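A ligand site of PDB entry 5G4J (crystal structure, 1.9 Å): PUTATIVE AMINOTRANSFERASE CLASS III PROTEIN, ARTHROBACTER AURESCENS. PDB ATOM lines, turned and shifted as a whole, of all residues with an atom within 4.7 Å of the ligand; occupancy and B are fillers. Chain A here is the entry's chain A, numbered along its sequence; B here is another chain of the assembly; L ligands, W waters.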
ATOM      1  N   TYR A  61      32.560  17.497  13.913  1.00  0.00           N
ATOM      2  CA  TYR A  61      31.387  18.384  13.908  1.00  0.00           C
ATOM      3  C   TYR A  61      30.739  18.715  15.236  1.00  0.00           C
ATOM      4  O   TYR A  61      30.246  19.828  15.360  1.00  0.00           O
ATOM      5  CB  TYR A  61      30.251  17.813  12.960  1.00  0.00           C
ATOM      6  CG  TYR A  61      29.060  18.799  12.934  1.00  0.00           C
ATOM      7  CD1 TYR A  61      29.193  20.006  12.271  1.00  0.00           C
ATOM      8  CD2 TYR A  61      27.876  18.583  13.649  1.00  0.00           C
ATOM      9  CE1 TYR A  61      28.200  20.944  12.250  1.00  0.00           C
ATOM     10  CE2 TYR A  61      26.827  19.544  13.642  1.00  0.00           C
ATOM     11  CZ  TYR A  61      26.999  20.760  12.920  1.00  0.00           C
ATOM     12  OH  TYR A  61      26.107  21.870  12.731  1.00  0.00           O
ATOM     13  N   ASN A  63      30.016  19.687  18.964  1.00  0.00           N
ATOM     14  CA  ASN A  63      30.527  20.420  20.088  1.00  0.00           C
ATOM     15  C   ASN A  63      29.880  20.117  21.384  1.00  0.00           C
ATOM     16  O   ASN A  63      30.399  20.485  22.412  1.00  0.00           O
ATOM     17  CB  ASN A  63      30.523  21.921  19.819  1.00  0.00           C
ATOM     18  CG  ASN A  63      29.137  22.508  19.754  1.00  0.00           C
ATOM     19  OD1 ASN A  63      28.175  21.837  19.439  1.00  0.00           O
ATOM     20  ND2 ASN A  63      29.079  23.786  20.008  1.00  0.00           N
ATOM     21  N   SER A 119      18.949  24.889  28.923  1.00  0.00           N
ATOM     22  CA  SER A 119      19.285  24.930  27.505  1.00  0.00           C
ATOM     23  C   SER A 119      19.776  26.326  27.142  1.00  0.00           C
ATOM     24  O   SER A 119      19.544  27.322  27.865  1.00  0.00           O
ATOM     25  CB  SER A 119      18.038  24.648  26.629  1.00  0.00           C
ATOM     26  OG  SER A 119      17.051  25.672  26.787  1.00  0.00           O
ATOM     27  N   GLY A 120      20.430  26.377  26.019  1.00  0.00           N
ATOM     28  CA  GLY A 120      20.805  27.616  25.391  1.00  0.00           C
ATOM     29  C   GLY A 120      19.604  28.515  25.064  1.00  0.00           C
ATOM     30  O   GLY A 120      19.695  29.766  25.292  1.00  0.00           O
ATOM     31  N   SER A 121      18.491  27.977  24.536  1.00  0.00           N
ATOM     32  CA  SER A 121      17.283  28.777  24.312  1.00  0.00           C
ATOM     33  C   SER A 121      16.777  29.363  25.596  1.00  0.00           C
ATOM     34  O   SER A 121      16.435  30.544  25.624  1.00  0.00           O
ATOM     35  CB  SER A 121      16.115  28.046  23.563  1.00  0.00           C
ATOM     36  OG  SER A 121      16.565  27.660  22.263  1.00  0.00           O
ATOM     37  N   ASN A 124      19.089  32.387  26.491  1.00  0.00           N
ATOM     38  CA  ASN A 124      18.885  33.570  25.672  1.00  0.00           C
ATOM     39  C   ASN A 124      17.528  34.187  25.957  1.00  0.00           C
ATOM     40  O   ASN A 124      17.415  35.408  25.956  1.00  0.00           O
ATOM     41  CB  ASN A 124      19.036  33.270  24.207  1.00  0.00           C
ATOM     42  CG  ASN A 124      20.507  33.246  23.762  1.00  0.00           C
ATOM     43  OD1 ASN A 124      21.355  33.957  24.318  1.00  0.00           O
ATOM     44  ND2 ASN A 124      20.799  32.438  22.769  1.00  0.00           N
ATOM     45  N   TYR A 147      20.829  32.700  14.566  1.00  0.00           N
ATOM     46  CA  TYR A 147      19.917  31.775  15.248  1.00  0.00           C
ATOM     47  C   TYR A 147      20.322  31.662  16.729  1.00  0.00           C
ATOM     48  O   TYR A 147      21.441  31.285  17.039  1.00  0.00           O
ATOM     49  CB  TYR A 147      19.913  30.402  14.674  1.00  0.00           C
ATOM     50  CG  TYR A 147      19.029  29.469  15.416  1.00  0.00           C
ATOM     51  CD1 TYR A 147      17.633  29.634  15.391  1.00  0.00           C
ATOM     52  CD2 TYR A 147      19.563  28.436  16.205  1.00  0.00           C
ATOM     53  CE1 TYR A 147      16.796  28.817  16.106  1.00  0.00           C
ATOM     54  CE2 TYR A 147      18.685  27.600  16.974  1.00  0.00           C
ATOM     55  CZ  TYR A 147      17.334  27.778  16.907  1.00  0.00           C
ATOM     56  OH  TYR A 147      16.448  27.005  17.635  1.00  0.00           O
ATOM     57  N   HIS A 148      19.400  32.066  17.613  1.00  0.00           N
ATOM     58  CA  HIS A 148      19.735  32.110  19.055  1.00  0.00           C
ATOM     59  C   HIS A 148      18.799  31.252  19.892  1.00  0.00           C
ATOM     60  O   HIS A 148      18.874  31.299  21.123  1.00  0.00           O
ATOM     61  CB  HIS A 148      19.718  33.549  19.510  1.00  0.00           C
ATOM     62  CG  HIS A 148      20.738  34.375  18.851  1.00  0.00           C
ATOM     63  ND1 HIS A 148      22.077  34.252  19.147  1.00  0.00           N
ATOM     64  CD2 HIS A 148      20.666  35.283  17.845  1.00  0.00           C
ATOM     65  CE1 HIS A 148      22.773  35.103  18.416  1.00  0.00           C
ATOM     66  NE2 HIS A 148      21.940  35.694  17.564  1.00  0.00           N
ATOM     67  N   GLY A 149      17.891  30.530  19.227  1.00  0.00           N
ATOM     68  CA  GLY A 149      16.982  29.614  19.962  1.00  0.00           C
ATOM     69  C   GLY A 149      15.579  29.604  19.510  1.00  0.00           C
ATOM     70  O   GLY A 149      15.201  30.285  18.529  1.00  0.00           O
ATOM     71  N   ASN A 150      14.761  28.884  20.223  1.00  0.00           N
ATOM     72  CA  ASN A 150      13.462  28.418  19.681  1.00  0.00           C
ATOM     73  C   ASN A 150      12.191  28.798  20.438  1.00  0.00           C
ATOM     74  O   ASN A 150      11.130  28.170  20.228  1.00  0.00           O
ATOM     75  CB  ASN A 150      13.537  26.861  19.584  1.00  0.00           C
ATOM     76  CG  ASN A 150      13.820  26.230  20.902  1.00  0.00           C
ATOM     77  OD1 ASN A 150      13.315  26.693  21.938  1.00  0.00           O
ATOM     78  ND2 ASN A 150      14.638  25.177  20.905  1.00  0.00           N
ATOM     79  N   ASP A 218      26.658  36.004  18.319  1.00  0.00           N
ATOM     80  CA  ASP A 218      27.608  34.884  18.416  1.00  0.00           C
ATOM     81  C   ASP A 218      28.974  35.442  17.999  1.00  0.00           C
ATOM     82  O   ASP A 218      29.153  35.791  16.850  1.00  0.00           O
ATOM     83  CB  ASP A 218      27.174  33.723  17.521  1.00  0.00           C
ATOM     84  CG  ASP A 218      28.317  32.712  17.165  1.00  0.00           C
ATOM     85  OD1 ASP A 218      29.339  32.645  17.897  1.00  0.00           O
ATOM     86  OD2 ASP A 218      28.175  32.034  16.117  1.00  0.00           O
ATOM     87  N   ASP A 251      26.383  35.552  23.051  1.00  0.00           N
ATOM     88  CA  ASP A 251      25.857  34.182  22.986  1.00  0.00           C
ATOM     89  C   ASP A 251      27.070  33.291  22.712  1.00  0.00           C
ATOM     90  O   ASP A 251      27.617  33.297  21.647  1.00  0.00           O
ATOM     91  CB  ASP A 251      24.838  34.096  21.875  1.00  0.00           C
ATOM     92  CG  ASP A 251      24.277  32.688  21.682  1.00  0.00           C
ATOM     93  OD1 ASP A 251      24.890  31.713  22.141  1.00  0.00           O
ATOM     94  OD2 ASP A 251      23.169  32.578  21.077  1.00  0.00           O
ATOM     95  N   VAL A 253      27.130  29.907  22.932  1.00  0.00           N
ATOM     96  CA  VAL A 253      26.746  28.523  22.711  1.00  0.00           C
ATOM     97  C   VAL A 253      27.718  27.867  21.689  1.00  0.00           C
ATOM     98  O   VAL A 253      28.066  26.706  21.816  1.00  0.00           O
ATOM     99  CB  VAL A 253      25.285  28.415  22.274  1.00  0.00           C
ATOM    100  CG1 VAL A 253      24.973  27.091  21.744  1.00  0.00           C
ATOM    101  CG2 VAL A 253      24.359  28.777  23.428  1.00  0.00           C
ATOM    102  N   GLN A 254      28.160  28.614  20.687  1.00  0.00           N
ATOM    103  CA  GLN A 254      29.100  28.123  19.696  1.00  0.00           C
ATOM    104  C   GLN A 254      30.567  28.449  20.037  1.00  0.00           C
ATOM    105  O   GLN A 254      31.469  27.643  19.627  1.00  0.00           O
ATOM    106  CB  GLN A 254      28.836  28.742  18.300  1.00  0.00           C
ATOM    107  CG  GLN A 254      27.495  28.410  17.738  1.00  0.00           C
ATOM    108  CD  GLN A 254      27.325  26.975  17.351  1.00  0.00           C
ATOM    109  OE1 GLN A 254      28.290  26.285  17.113  1.00  0.00           O
ATOM    110  NE2 GLN A 254      26.093  26.494  17.354  1.00  0.00           N
ATOM    111  N   LYS A 281      25.154  24.340  24.958  1.00  0.00           N
ATOM    112  CA  LYS A 281      25.841  23.134  24.341  1.00  0.00           C
ATOM    113  C   LYS A 281      26.815  22.272  25.146  1.00  0.00           C
ATOM    114  O   LYS A 281      26.401  21.394  25.912  1.00  0.00           O
ATOM    115  CB  LYS A 281      26.314  23.451  22.933  1.00  0.00           C
ATOM    116  CG  LYS A 281      25.130  23.475  21.942  1.00  0.00           C
ATOM    117  CD  LYS A 281      25.536  24.044  20.579  1.00  0.00           C
ATOM    118  CE  LYS A 281      24.332  24.206  19.628  1.00  0.00           C
ATOM    119  NZ  LYS A 281      23.612  23.047  19.058  1.00  0.00           N
ATOM    120  N   LYS A 412      31.863  23.545   7.916  1.00  0.00           N
ATOM    121  CA  LYS A 412      31.940  23.843   9.349  1.00  0.00           C
ATOM    122  C   LYS A 412      32.570  22.595  10.050  1.00  0.00           C
ATOM    123  O   LYS A 412      31.968  21.513  10.052  1.00  0.00           O
ATOM    124  CB  LYS A 412      30.536  24.078   9.920  1.00  0.00           C
ATOM    125  CG  LYS A 412      30.336  23.845  11.437  1.00  0.00           C
ATOM    126  CD  LYS A 412      29.235  24.694  12.054  1.00  0.00           C
ATOM    127  CE  LYS A 412      27.987  24.058  12.590  1.00  0.00           C
ATOM    128  NZ  LYS A 412      27.168  25.107  13.351  1.00  0.00           N
ATOM    129  N   ARG A 414      34.189  21.418  13.743  1.00  0.00           N
ATOM    130  CA  ARG A 414      33.947  21.871  15.133  1.00  0.00           C
ATOM    131  C   ARG A 414      33.923  20.648  15.981  1.00  0.00           C
ATOM    132  O   ARG A 414      32.881  20.300  16.532  1.00  0.00           O
ATOM    133  CB  ARG A 414      32.648  22.640  15.207  1.00  0.00           C
ATOM    134  CG  ARG A 414      32.308  23.292  16.546  1.00  0.00           C
ATOM    135  CD  ARG A 414      30.802  23.638  16.589  1.00  0.00           C
ATOM    136  NE  ARG A 414      29.977  22.489  16.325  1.00  0.00           N
ATOM    137  CZ  ARG A 414      28.647  22.538  16.222  1.00  0.00           C
ATOM    138  NH1 ARG A 414      27.971  23.664  16.491  1.00  0.00           N
ATOM    139  NH2 ARG A 414      27.960  21.439  15.883  1.00  0.00           N
ATOM    140  N   ARG B  90      19.670  14.888  15.332  1.00  0.00           N
ATOM    141  CA  ARG B  90      20.063  14.874  13.901  1.00  0.00           C
ATOM    142  C   ARG B  90      20.808  13.619  13.406  1.00  0.00           C
ATOM    143  O   ARG B  90      20.997  13.434  12.171  1.00  0.00           O
ATOM    144  CB  ARG B  90      20.754  16.173  13.503  1.00  0.00           C
ATOM    145  CG  ARG B  90      19.843  17.382  13.747  1.00  0.00           C
ATOM    146  CD  ARG B  90      20.561  18.720  13.629  1.00  0.00           C
ATOM    147  NE  ARG B  90      21.602  18.821  14.649  1.00  0.00           N
ATOM    148  CZ  ARG B  90      22.456  19.864  14.794  1.00  0.00           C
ATOM    149  NH1 ARG B  90      22.409  20.904  13.983  1.00  0.00           N
ATOM    150  NH2 ARG B  90      23.403  19.821  15.745  1.00  0.00           N
ATOM    151  N   PHE B 309      14.110  22.990  16.226  1.00  0.00           N
ATOM    152  CA  PHE B 309      15.113  22.068  16.761  1.00  0.00           C
ATOM    153  C   PHE B 309      15.498  22.527  18.169  1.00  0.00           C
ATOM    154  O   PHE B 309      15.697  23.721  18.423  1.00  0.00           O
ATOM    155  CB  PHE B 309      16.344  22.064  15.834  1.00  0.00           C
ATOM    156  CG  PHE B 309      17.491  21.194  16.310  1.00  0.00           C
ATOM    157  CD1 PHE B 309      17.316  19.822  16.483  1.00  0.00           C
ATOM    158  CD2 PHE B 309      18.738  21.765  16.600  1.00  0.00           C
ATOM    159  CE1 PHE B 309      18.390  19.040  16.952  1.00  0.00           C
ATOM    160  CE2 PHE B 309      19.809  20.989  17.082  1.00  0.00           C
ATOM    161  CZ  PHE B 309      19.622  19.626  17.263  1.00  0.00           C
ATOM    162  N   ASN B 310      15.610  21.562  19.067  1.00  0.00           N
ATOM    163  CA  ASN B 310      16.013  21.838  20.489  1.00  0.00           C
ATOM    164  C   ASN B 310      17.218  20.960  20.742  1.00  0.00           C
ATOM    165  O   ASN B 310      17.070  19.703  20.720  1.00  0.00           O
ATOM    166  CB  ASN B 310      14.804  21.469  21.360  1.00  0.00           C
ATOM    167  CG  ASN B 310      15.088  21.581  22.836  1.00  0.00           C
ATOM    168  OD1 ASN B 310      16.214  21.214  23.297  1.00  0.00           O
ATOM    169  ND2 ASN B 310      14.042  22.031  23.622  1.00  0.00           N
ATOM    170  N   THR B 311      18.410  21.555  20.915  1.00  0.00           N
ATOM    171  CA  THR B 311      19.698  20.787  20.895  1.00  0.00           C
ATOM    172  C   THR B 311      19.735  19.551  21.855  1.00  0.00           C
ATOM    173  O   THR B 311      20.163  18.477  21.436  1.00  0.00           O
ATOM    174  CB  THR B 311      20.928  21.702  21.232  1.00  0.00           C
ATOM    175  OG1 THR B 311      21.074  22.728  20.198  1.00  0.00           O
ATOM    176  CG2 THR B 311      22.206  20.855  21.418  1.00  0.00           C
ATOM    177  N   PHE B 312      19.272  19.743  23.100  1.00  0.00           N
ATOM    178  CA  PHE B 312      19.347  18.666  24.139  1.00  0.00           C
ATOM    179  C   PHE B 312      18.124  17.759  24.133  1.00  0.00           C
ATOM    180  O   PHE B 312      18.180  16.585  24.671  1.00  0.00           O
ATOM    181  CB  PHE B 312      19.443  19.257  25.524  1.00  0.00           C
ATOM    182  CG  PHE B 312      20.739  20.065  25.737  1.00  0.00           C
ATOM    183  CD1 PHE B 312      21.986  19.573  25.296  1.00  0.00           C
ATOM    184  CD2 PHE B 312      20.693  21.329  26.375  1.00  0.00           C
ATOM    185  CE1 PHE B 312      23.202  20.302  25.508  1.00  0.00           C
ATOM    186  CE2 PHE B 312      21.892  22.030  26.579  1.00  0.00           C
ATOM    187  CZ  PHE B 312      23.164  21.494  26.182  1.00  0.00           C
HETATM  188  C1  LIG L   1      21.916  27.488  19.376  1.00  0.00           C
HETATM  189  C2  LIG L   1      21.560  26.211  18.851  1.00  0.00           C
HETATM  190  P1  LIG L   1      19.525  25.120  22.380  1.00  0.00           P
HETATM  191  O1  LIG L   1      19.164  24.463  21.066  1.00  0.00           O
HETATM  192  O2  LIG L   1      20.139  24.390  23.434  1.00  0.00           O
HETATM  193  O3  LIG L   1      18.245  25.630  22.990  1.00  0.00           O
HETATM  194  O4  LIG L   1      20.438  26.285  22.052  1.00  0.00           O
HETATM  195  C3  LIG L   1      20.139  27.431  21.192  1.00  0.00           C
HETATM  196  C4  LIG L   1      21.228  28.066  20.499  1.00  0.00           C
HETATM  197  N1  LIG L   1      22.580  30.119  20.332  1.00  0.00           N
HETATM  198  C5  LIG L   1      21.583  29.378  20.893  1.00  0.00           C
HETATM  199  C6  LIG L   1      23.242  29.582  19.246  1.00  0.00           C
HETATM  200  C7  LIG L   1      24.257  30.387  18.636  1.00  0.00           C
HETATM  201  C8  LIG L   1      22.913  28.298  18.757  1.00  0.00           C
HETATM  202  O5  LIG L   1      23.599  27.819  17.658  1.00  0.00           O
HETATM  203  O6  LIG L   1      25.553  24.338  15.600  1.00  0.00           O
HETATM  204  P2  LIG L   1      24.635  23.064  15.598  1.00  0.00           P
HETATM  205  O7  LIG L   1      24.187  22.750  14.125  1.00  0.00           O
HETATM  206  O8  LIG L   1      25.249  21.791  16.186  1.00  0.00           O
HETATM  207  O9  LIG L   1      23.242  23.539  16.421  1.00  0.00           O
HETATM  208  C9  LIG L   1      22.138  24.168  15.806  1.00  0.00           C
HETATM  209  C10 LIG L   1      21.277  24.615  17.002  1.00  0.00           C
HETATM  210  N2  LIG L   1      21.943  25.797  17.659  1.00  0.00           N
HETATM  211  O   HOH W   1      23.158  29.866  15.501  1.00  0.00           O
HETATM  212  O   HOH W   2      18.736  22.313  24.019  1.00  0.00           O
HETATM  213  O   HOH W   3      16.020  24.277  23.424  1.00  0.00           O
HETATM  214  O   HOH W   4      24.629  24.634  12.506  1.00  0.00           O
HETATM  215  O   HOH W   5      22.668  24.958  23.710  1.00  0.00           O
HETATM  216  O   HOH W   6      25.739  21.057  18.691  1.00  0.00           O
HETATM  217  O   HOH W   7      17.865  25.139  19.012  1.00  0.00           O
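The backbone NH (N) of Gly 120 sits at hydrogen-bond distance from an oxygen (O2) of the ligand. The side-chain hydroxyl of Ser 121 lies within hydrogen-bond range of an oxygen (O3) of the ligand. The side-chain amino group (NZ) of Lys 412 is in salt-bridge range of an oxygen (O6) of the ligand (2.9 Å). The backbone NH (N) of Thr 311 of chain B is in hydrogen-bond range of an oxygen (O1) of the ligand (3.0 Å). The guanidinium group of Arg 90 of chain B lies within salt-bridge range of an oxygen (O7) of the ligand (2.6 Å). NZ of Lys 281 is in salt-bridge range of O8 of the ligand (3.5 Å). N1 of the ligand sits at hydrogen-bond distance from OD2 of Asp 251. The side-chain hydroxyl (OG1) of Thr 311 of chain B is in hydrogen-bond range of an oxygen (O1) of the ligand (2.7 Å). An oxygen (O3) of the ligand lies within hydrogen-bond range of the backbone NH (N) of Ser 121, 2.8 Å away. The guanidinium group (NH1) of Arg 414 lies within salt-bridge range of an oxygen (O6) of the ligand (2.7 Å). OH of Tyr 61 lies within hydrogen-bond range of O7 of the ligand, at 2.5 Å. O6 of the ligand is in hydrogen-bond range of NE2 of Gln 254 (2.8 Å).
The side-chain hydroxyl (OG) of Ser 121 is in hydrogen-bond range of the backbone NH (N) of Asn 150 (3.0 Å). The backbone NH (N) of Val 253 lies within hydrogen-bond range of the side-chain carboxylate (OD1) of Asp 251 (3.0 Å). A ring nitrogen (ND1) of His 148 is in hydrogen-bond range of the side-chain carboxylate (OD2) of Asp 251 (2.8 Å). The side-chain amino group (NZ) of Lys 281 lies within hydrogen-bond range of the side-chain hydroxyl (OG1) of Thr 311 of chain B (2.8 Å). O of Tyr 61 lies within hydrogen-bond range of NE of Arg 414, at 2.8 Å. The guanidinium group (NH1) of Arg 414 lies within hydrogen-bond range of the side-chain amide oxygen (OE1) of Gln 254, at 2.7 Å. The guanidinium group (NH1) of Arg 414 lies close to the side-chain amide oxygen (OD1) of Asn 63. The side-chain carboxylate (OD2) of Asp 251 is in hydrogen-bond range of the side-chain amide nitrogen (ND2) of Asn 124.
Merely in contact with the ligand: Tyr 147 (3.3 Å), His 148 (3.3 Å), Asn 124 (3.7 Å), Val 253 (3.7 Å), Ser 119 (3.8 Å) and Phe 309 of chain B (3.8 Å). Hydrophobic or aromatic side chains within 4 Å of the ligand: Tyr 61, Tyr 147, Val 253 and Phe 309 of chain B. Of the 22 residues printed, 16 come within 4 Å of the ligand. The nearest printed residue that does not touch the ligand is Asn 310 of chain B (4.02 Å).
Water W4 lies within hydrogen-bond range of O7 of the ligand (2.5 Å), NZ of Lys 412 (2.7 Å) and OH of Tyr 61 (3.1 Å). Water W2 lies within hydrogen-bond range of an oxygen (O2) of the ligand (2.6 Å), the backbone NH of Phe 312 of chain B (2.8 Å), the side-chain amide oxygen of Asn 310 of chain B (2.8 Å) and the backbone NH of Thr 311 of chain B (3.2 Å). Water W5 bridges O2 of the ligand (2.6 Å) and N of Lys 281 (2.8 Å). Water W3 lies within hydrogen-bond range of O3 of the ligand (2.6 Å), ND2 of Asn 310 of chain B (3.0 Å) and ND2 of Asn 150 (3.0 Å). Water W6 lies within hydrogen-bond range of an oxygen (O8) of the ligand (2.7 Å), the side-chain amide oxygen of Asn 63 (2.7 Å) and the side-chain amino group of Lys 281 (2.9 Å). Water W1 lies within hydrogen-bond range of the backbone carbonyl oxygen of Tyr 147 (2.7 Å) and an oxygen (O5) of the ligand (3.0 Å).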
